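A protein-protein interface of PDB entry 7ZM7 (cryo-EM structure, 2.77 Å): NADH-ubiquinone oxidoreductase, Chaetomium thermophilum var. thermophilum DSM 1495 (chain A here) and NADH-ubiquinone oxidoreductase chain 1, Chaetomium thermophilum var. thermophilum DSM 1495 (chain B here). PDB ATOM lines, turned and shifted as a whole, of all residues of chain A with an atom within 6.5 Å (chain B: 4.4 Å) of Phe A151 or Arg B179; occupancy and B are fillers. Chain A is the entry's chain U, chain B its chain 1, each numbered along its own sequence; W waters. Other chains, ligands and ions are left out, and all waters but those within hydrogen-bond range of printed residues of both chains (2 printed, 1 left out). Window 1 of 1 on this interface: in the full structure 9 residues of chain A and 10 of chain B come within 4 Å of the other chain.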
ATOM      1  N   GLN A 108      37.329   6.086  33.993  1.00  0.00           N
ATOM      2  CA  GLN A 108      36.754   6.910  32.888  1.00  0.00           C
ATOM      3  C   GLN A 108      35.987   8.071  33.529  1.00  0.00           C
ATOM      4  O   GLN A 108      35.096   7.791  34.331  1.00  0.00           O
ATOM      5  CB  GLN A 108      35.972   6.047  31.896  1.00  0.00           C
ATOM      6  CG  GLN A 108      36.813   4.965  31.239  1.00  0.00           C
ATOM      7  CD  GLN A 108      35.978   4.000  30.435  1.00  0.00           C
ATOM      8  OE1 GLN A 108      34.770   3.915  30.602  1.00  0.00           O
ATOM      9  NE2 GLN A 108      36.622   3.261  29.550  1.00  0.00           N
ATOM     10  N   TRP A 110      33.734  10.336  32.492  1.00  0.00           N
ATOM     11  CA  TRP A 110      32.302  10.523  32.165  1.00  0.00           C
ATOM     12  C   TRP A 110      31.441   9.584  33.014  1.00  0.00           C
ATOM     13  O   TRP A 110      30.211   9.738  32.997  1.00  0.00           O
ATOM     14  CB  TRP A 110      32.082  10.320  30.664  1.00  0.00           C
ATOM     15  CG  TRP A 110      32.488   8.991  30.109  1.00  0.00           C
ATOM     16  CD1 TRP A 110      31.708   7.881  29.980  1.00  0.00           C
ATOM     17  CD2 TRP A 110      33.765   8.646  29.542  1.00  0.00           C
ATOM     18  NE1 TRP A 110      32.416   6.866  29.398  1.00  0.00           N
ATOM     19  CE2 TRP A 110      33.679   7.306  29.116  1.00  0.00           C
ATOM     20  CE3 TRP A 110      34.972   9.331  29.368  1.00  0.00           C
ATOM     21  CZ2 TRP A 110      34.750   6.646  28.517  1.00  0.00           C
ATOM     22  CZ3 TRP A 110      36.029   8.678  28.779  1.00  0.00           C
ATOM     23  CH2 TRP A 110      35.919   7.352  28.365  1.00  0.00           C
ATOM     24  N   GLN A 111      32.061   8.644  33.724  1.00  0.00           N
ATOM     25  CA  GLN A 111      31.295   7.629  34.483  1.00  0.00           C
ATOM     26  C   GLN A 111      31.058   8.071  35.934  1.00  0.00           C
ATOM     27  O   GLN A 111      30.372   7.323  36.648  1.00  0.00           O
ATOM     28  CB  GLN A 111      32.001   6.284  34.423  1.00  0.00           C
ATOM     29  CG  GLN A 111      32.561   5.955  33.052  1.00  0.00           C
ATOM     30  CD  GLN A 111      31.789   4.871  32.344  1.00  0.00           C
ATOM     31  OE1 GLN A 111      30.619   5.031  32.017  1.00  0.00           O
ATOM     32  NE2 GLN A 111      32.449   3.756  32.093  1.00  0.00           N
ATOM     33  N   GLN A 149      25.363  12.091  29.841  1.00  0.00           N
ATOM     34  CA  GLN A 149      26.602  11.517  29.263  1.00  0.00           C
ATOM     35  C   GLN A 149      26.172  10.267  28.516  1.00  0.00           C
ATOM     36  O   GLN A 149      25.656   9.348  29.154  1.00  0.00           O
ATOM     37  CB  GLN A 149      27.646  11.209  30.340  1.00  0.00           C
ATOM     38  CG  GLN A 149      28.226  12.436  31.026  1.00  0.00           C
ATOM     39  CD  GLN A 149      28.978  13.363  30.104  1.00  0.00           C
ATOM     40  OE1 GLN A 149      29.711  12.939  29.217  1.00  0.00           O
ATOM     41  NE2 GLN A 149      28.810  14.655  30.326  1.00  0.00           N
ATOM     42  N   ILE A 150      26.342  10.277  27.197  1.00  0.00           N
ATOM     43  CA  ILE A 150      25.870   9.153  26.347  1.00  0.00           C
ATOM     44  C   ILE A 150      26.638   7.888  26.712  1.00  0.00           C
ATOM     45  O   ILE A 150      26.011   6.828  26.805  1.00  0.00           O
ATOM     46  CB  ILE A 150      26.108   9.536  24.871  1.00  0.00           C
ATOM     47  CG1 ILE A 150      25.181  10.657  24.400  1.00  0.00           C
ATOM     48  CG2 ILE A 150      26.049   8.327  23.952  1.00  0.00           C
ATOM     49  CD1 ILE A 150      25.570  11.248  23.065  1.00  0.00           C
ATOM     50  N   PHE A 151      27.948   8.007  26.921  1.00  0.00           N
ATOM     51  CA  PHE A 151      28.773   6.796  27.107  1.00  0.00           C
ATOM     52  C   PHE A 151      28.832   6.367  28.568  1.00  0.00           C
ATOM     53  O   PHE A 151      29.538   5.392  28.860  1.00  0.00           O
ATOM     54  CB  PHE A 151      30.102   6.964  26.376  1.00  0.00           C
ATOM     55  CG  PHE A 151      29.969   7.182  24.892  1.00  0.00           C
ATOM     56  CD1 PHE A 151      29.765   6.114  24.035  1.00  0.00           C
ATOM     57  CD2 PHE A 151      30.034   8.456  24.354  1.00  0.00           C
ATOM     58  CE1 PHE A 151      29.634   6.314  22.672  1.00  0.00           C
ATOM     59  CE2 PHE A 151      29.903   8.656  22.991  1.00  0.00           C
ATOM     60  CZ  PHE A 151      29.704   7.584  22.153  1.00  0.00           C
ATOM     61  N   ALA A 152      28.093   7.049  29.448  1.00  0.00           N
ATOM     62  CA  ALA A 152      28.014   6.613  30.864  1.00  0.00           C
ATOM     63  C   ALA A 152      27.274   5.278  30.948  1.00  0.00           C
ATOM     64  O   ALA A 152      26.300   5.101  30.211  1.00  0.00           O
ATOM     65  CB  ALA A 152      27.339   7.658  31.699  1.00  0.00           C
ATOM     66  N   HIS A 153      27.713   4.386  31.834  1.00  0.00           N
ATOM     67  CA  HIS A 153      27.105   3.036  31.963  1.00  0.00           C
ATOM     68  C   HIS A 153      25.853   3.176  32.804  1.00  0.00           C
ATOM     69  O   HIS A 153      24.884   2.454  32.541  1.00  0.00           O
ATOM     70  CB  HIS A 153      28.079   2.101  32.673  1.00  0.00           C
ATOM     71  CG  HIS A 153      29.239   1.671  31.843  1.00  0.00           C
ATOM     72  ND1 HIS A 153      30.024   0.596  32.187  1.00  0.00           N
ATOM     73  CD2 HIS A 153      29.744   2.156  30.691  1.00  0.00           C
ATOM     74  CE1 HIS A 153      30.966   0.438  31.283  1.00  0.00           C
ATOM     75  NE2 HIS A 153      30.820   1.384  30.361  1.00  0.00           N
ATOM     76  N   HIS A 154      25.885   4.099  33.765  1.00  0.00           N
ATOM     77  CA  HIS A 154      24.703   4.391  34.612  1.00  0.00           C
ATOM     78  C   HIS A 154      24.254   5.822  34.314  1.00  0.00           C
ATOM     79  O   HIS A 154      25.127   6.688  34.156  1.00  0.00           O
ATOM     80  CB  HIS A 154      25.048   4.191  36.091  1.00  0.00           C
ATOM     81  CG  HIS A 154      25.720   2.887  36.357  1.00  0.00           C
ATOM     82  ND1 HIS A 154      25.042   1.685  36.304  1.00  0.00           N
ATOM     83  CD2 HIS A 154      27.001   2.587  36.662  1.00  0.00           C
ATOM     84  CE1 HIS A 154      25.876   0.701  36.570  1.00  0.00           C
ATOM     85  NE2 HIS A 154      27.085   1.228  36.794  1.00  0.00           N
ATOM     86  N   PRO B 100      31.741  -5.179  29.737  1.00  0.00           N
ATOM     87  CA  PRO B 100      32.934  -4.452  29.316  1.00  0.00           C
ATOM     88  C   PRO B 100      34.220  -5.145  29.774  1.00  0.00           C
ATOM     89  O   PRO B 100      34.414  -5.254  30.940  1.00  0.00           O
ATOM     90  CB  PRO B 100      32.756  -3.102  30.004  1.00  0.00           C
ATOM     91  CG  PRO B 100      31.265  -2.995  30.231  1.00  0.00           C
ATOM     92  CD  PRO B 100      30.845  -4.404  30.582  1.00  0.00           C
ATOM     93  N   VAL B 175      31.422  -2.582  20.935  1.00  0.00           N
ATOM     94  CA  VAL B 175      30.097  -2.599  21.626  1.00  0.00           C
ATOM     95  C   VAL B 175      29.902  -1.292  22.386  1.00  0.00           C
ATOM     96  O   VAL B 175      28.824  -0.703  22.267  1.00  0.00           O
ATOM     97  CB  VAL B 175      29.928  -3.821  22.550  1.00  0.00           C
ATOM     98  CG1 VAL B 175      28.717  -3.695  23.454  1.00  0.00           C
ATOM     99  CG2 VAL B 175      29.884  -5.116  21.764  1.00  0.00           C
ATOM    100  N   GLU B 176      30.924  -0.835  23.093  1.00  0.00           N
ATOM    101  CA  GLU B 176      30.809   0.384  23.927  1.00  0.00           C
ATOM    102  C   GLU B 176      30.451   1.584  23.046  1.00  0.00           C
ATOM    103  O   GLU B 176      29.779   2.484  23.546  1.00  0.00           O
ATOM    104  CB  GLU B 176      32.129   0.565  24.676  1.00  0.00           C
ATOM    105  CG  GLU B 176      32.267  -0.368  25.860  1.00  0.00           C
ATOM    106  CD  GLU B 176      31.229  -0.113  26.933  1.00  0.00           C
ATOM    107  OE1 GLU B 176      30.555  -1.071  27.343  1.00  0.00           O
ATOM    108  OE2 GLU B 176      31.096   1.051  27.345  1.00  0.00           O
ATOM    109  N   SER B 177      30.916   1.568  21.795  1.00  0.00           N
ATOM    110  CA  SER B 177      30.686   2.663  20.823  1.00  0.00           C
ATOM    111  C   SER B 177      29.219   2.694  20.405  1.00  0.00           C
ATOM    112  O   SER B 177      28.769   3.738  19.916  1.00  0.00           O
ATOM    113  CB  SER B 177      31.587   2.456  19.640  1.00  0.00           C
ATOM    114  OG  SER B 177      32.949   2.483  20.031  1.00  0.00           O
ATOM    115  N   GLN B 178      28.501   1.601  20.635  1.00  0.00           N
ATOM    116  CA  GLN B 178      27.079   1.502  20.229  1.00  0.00           C
ATOM    117  C   GLN B 178      26.181   2.036  21.344  1.00  0.00           C
ATOM    118  O   GLN B 178      24.957   1.952  21.191  1.00  0.00           O
ATOM    119  CB  GLN B 178      26.779   0.077  19.782  1.00  0.00           C
ATOM    120  CG  GLN B 178      27.639  -0.364  18.609  1.00  0.00           C
ATOM    121  CD  GLN B 178      27.266  -1.737  18.117  1.00  0.00           C
ATOM    122  OE1 GLN B 178      26.126  -1.990  17.740  1.00  0.00           O
ATOM    123  NE2 GLN B 178      28.235  -2.635  18.110  1.00  0.00           N
ATOM    124  N   ARG B 179      26.767   2.546  22.425  1.00  0.00           N
ATOM    125  CA  ARG B 179      25.958   3.177  23.498  1.00  0.00           C
ATOM    126  C   ARG B 179      25.248   4.374  22.866  1.00  0.00           C
ATOM    127  O   ARG B 179      24.160   4.707  23.345  1.00  0.00           O
ATOM    128  CB  ARG B 179      26.801   3.471  24.741  1.00  0.00           C
ATOM    129  CG  ARG B 179      27.050   2.259  25.624  1.00  0.00           C
ATOM    130  CD  ARG B 179      27.731   2.598  26.936  1.00  0.00           C
ATOM    131  NE  ARG B 179      28.204   1.393  27.597  1.00  0.00           N
ATOM    132  CZ  ARG B 179      27.542   0.723  28.535  1.00  0.00           C
ATOM    133  NH1 ARG B 179      26.361   1.145  28.951  1.00  0.00           N
ATOM    134  NH2 ARG B 179      28.073  -0.369  29.055  1.00  0.00           N
ATOM    135  N   ALA B 180      25.876   5.035  21.888  1.00  0.00           N
ATOM    136  CA  ALA B 180      25.214   6.115  21.117  1.00  0.00           C
ATOM    137  C   ALA B 180      24.066   5.580  20.254  1.00  0.00           C
ATOM    138  O   ALA B 180      22.993   6.193  20.273  1.00  0.00           O
ATOM    139  CB  ALA B 180      26.239   6.767  20.229  1.00  0.00           C
ATOM    140  N   ILE B 181      24.284   4.481  19.535  1.00  0.00           N
ATOM    141  CA  ILE B 181      23.248   3.895  18.635  1.00  0.00           C
ATOM    142  C   ILE B 181      23.718   2.522  18.183  1.00  0.00           C
ATOM    143  O   ILE B 181      24.934   2.347  18.012  1.00  0.00           O
ATOM    144  CB  ILE B 181      22.966   4.795  17.411  1.00  0.00           C
ATOM    145  CG1 ILE B 181      21.644   4.442  16.726  1.00  0.00           C
ATOM    146  CG2 ILE B 181      24.130   4.780  16.433  1.00  0.00           C
ATOM    147  CD1 ILE B 181      20.421   4.823  17.523  1.00  0.00           C
ATOM    148  N   LEU B 256      24.647  -4.598  25.312  1.00  0.00           N
ATOM    149  CA  LEU B 256      24.002  -3.371  25.733  1.00  0.00           C
ATOM    150  C   LEU B 256      22.506  -3.572  25.874  1.00  0.00           C
ATOM    151  O   LEU B 256      21.812  -3.800  24.883  1.00  0.00           O
ATOM    152  CB  LEU B 256      24.294  -2.274  24.725  1.00  0.00           C
ATOM    153  CG  LEU B 256      25.682  -1.712  24.897  1.00  0.00           C
ATOM    154  CD1 LEU B 256      25.934  -0.641  23.871  1.00  0.00           C
ATOM    155  CD2 LEU B 256      25.794  -1.199  26.298  1.00  0.00           C
ATOM    156  N   TYR B 312      24.148  -8.200  31.524  1.00  0.00           N
ATOM    157  CA  TYR B 312      24.985  -7.954  30.328  1.00  0.00           C
ATOM    158  C   TYR B 312      25.026  -9.239  29.494  1.00  0.00           C
ATOM    159  O   TYR B 312      24.924  -9.153  28.260  1.00  0.00           O
ATOM    160  CB  TYR B 312      26.349  -7.382  30.723  1.00  0.00           C
ATOM    161  CG  TYR B 312      26.408  -5.891  30.928  1.00  0.00           C
ATOM    162  CD1 TYR B 312      25.409  -5.060  30.455  1.00  0.00           C
ATOM    163  CD2 TYR B 312      27.481  -5.305  31.576  1.00  0.00           C
ATOM    164  CE1 TYR B 312      25.466  -3.686  30.630  1.00  0.00           C
ATOM    165  CE2 TYR B 312      27.554  -3.936  31.764  1.00  0.00           C
ATOM    166  CZ  TYR B 312      26.541  -3.121  31.289  1.00  0.00           C
ATOM    167  OH  TYR B 312      26.606  -1.769  31.469  1.00  0.00           O
ATOM    168  N   LEU B 378      37.156   4.719  25.896  1.00  0.00           N
ATOM    169  CA  LEU B 378      36.055   3.716  25.849  1.00  0.00           C
ATOM    170  C   LEU B 378      36.559   2.275  26.006  1.00  0.00           C
ATOM    171  O   LEU B 378      35.920   1.372  25.439  1.00  0.00           O
ATOM    172  CB  LEU B 378      35.237   3.903  24.564  1.00  0.00           C
ATOM    173  CG  LEU B 378      33.875   4.569  24.740  1.00  0.00           C
ATOM    174  CD1 LEU B 378      34.007   6.080  24.806  1.00  0.00           C
ATOM    175  CD2 LEU B 378      32.951   4.174  23.607  1.00  0.00           C
HETATM  176  O   HOH W   1      31.619   3.604  28.312  1.00  0.00           O
HETATM  177  O   HOH W   2      24.460   3.702  27.751  1.00  0.00           O
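A ring nitrogen (NE2) of His A153 lies within hydrogen-bond range of the side-chain carboxylate (OE2) of Glu B176 (3.0 Å).
The guanidinium group (NE) of Arg B179 lies within salt-bridge range of the side-chain carboxylate (OE2) of Glu B176, at 2.9 Å. OE1 of Gln A111 sits close to O of Phe A151, at 3.4 Å. OE1 of Gln A108 sits at hydrogen-bond distance from NE2 of Gln A111 (2.8 Å). OH of Tyr B312 sits at hydrogen-bond distance from NH2 of Arg B179, 3.2 Å away. OE1 of Gln A111 is in hydrogen-bond range of N of His A153 (3.0 Å). The backbone carbonyl oxygen (O) of Phe A151 is in hydrogen-bond range of the indole nitrogen (NE1) of Trp A110, 3.3 Å away.
Among the printed residues, pairs that only touch across the chains: His A153 with Arg B179 (3.4 Å), His A153 with Pro B100 (3.6 Å), Phe A151 with Glu B176 (3.7 Å), Gln A108 with Leu B378 (3.7 Å), Ile A150 with Ala B180 (3.7 Å), Phe A151 with Leu B378 (3.8 Å), Trp A110 with Leu B378 (3.8 Å), Phe A151 with Arg B179 (3.8 Å) and Phe A151 with Ser B177 (3.9 Å).
Printed residues of chain B within 4 Å of Gln A108: Leu B378. Of the printed residues of chain B, Phe A151 touches Glu B176 (3.7 Å), Ser B177 (3.9 Å), Arg B179 (3.8 Å) and Leu B378 (3.8 Å). Val B175 touches none of the printed residues of chain A. Printed residues of chain A within 4 Å of Arg B179: Phe A151 (3.8 Å) and His A153 (3.4 Å). Leu B256 touches none of the printed residues of chain A. Of the printed residues of chain A, Leu B378 touches Gln A108 (3.7 Å), Trp A110 (3.8 Å) and Phe A151 (3.8 Å). The nearest printed residue of chain A that does not touch Arg B179 is Ile A150 (4.02 Å). The nearest printed residue of chain A that does not touch Glu B176 is Gln A111 (5.6 Å).
Of the 9 printed residues of chain A, 5 touch a printed residue of chain B. Hydrophobic or aromatic side chains of chain A that line the printed part of chain B: Trp A110, Ile A150, Phe A151 and His A153. Printed residues of chain B that touch a printed residue of chain A: Pro B100, Glu B176, Ser B177, Arg B179, Ala B180 and Leu B378. Hydrophobic or aromatic side chains of chain B within 4 Å of the printed part of chain A: Pro B100 and Leu B378. Among the printed residues, 10 pairs touch across the chains.
Water W1 lies within hydrogen-bond range of OE2 of Glu B176 (2.8 Å), O of Phe A151 (2.8 Å) and NE2 of His A153 (3.1 Å). Water W2 lies within hydrogen-bond range of the backbone carbonyl oxygen (O) of Ala A152 (3.4 Å) and the guanidinium group (NH1) of Arg B179 (3.4 Å).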
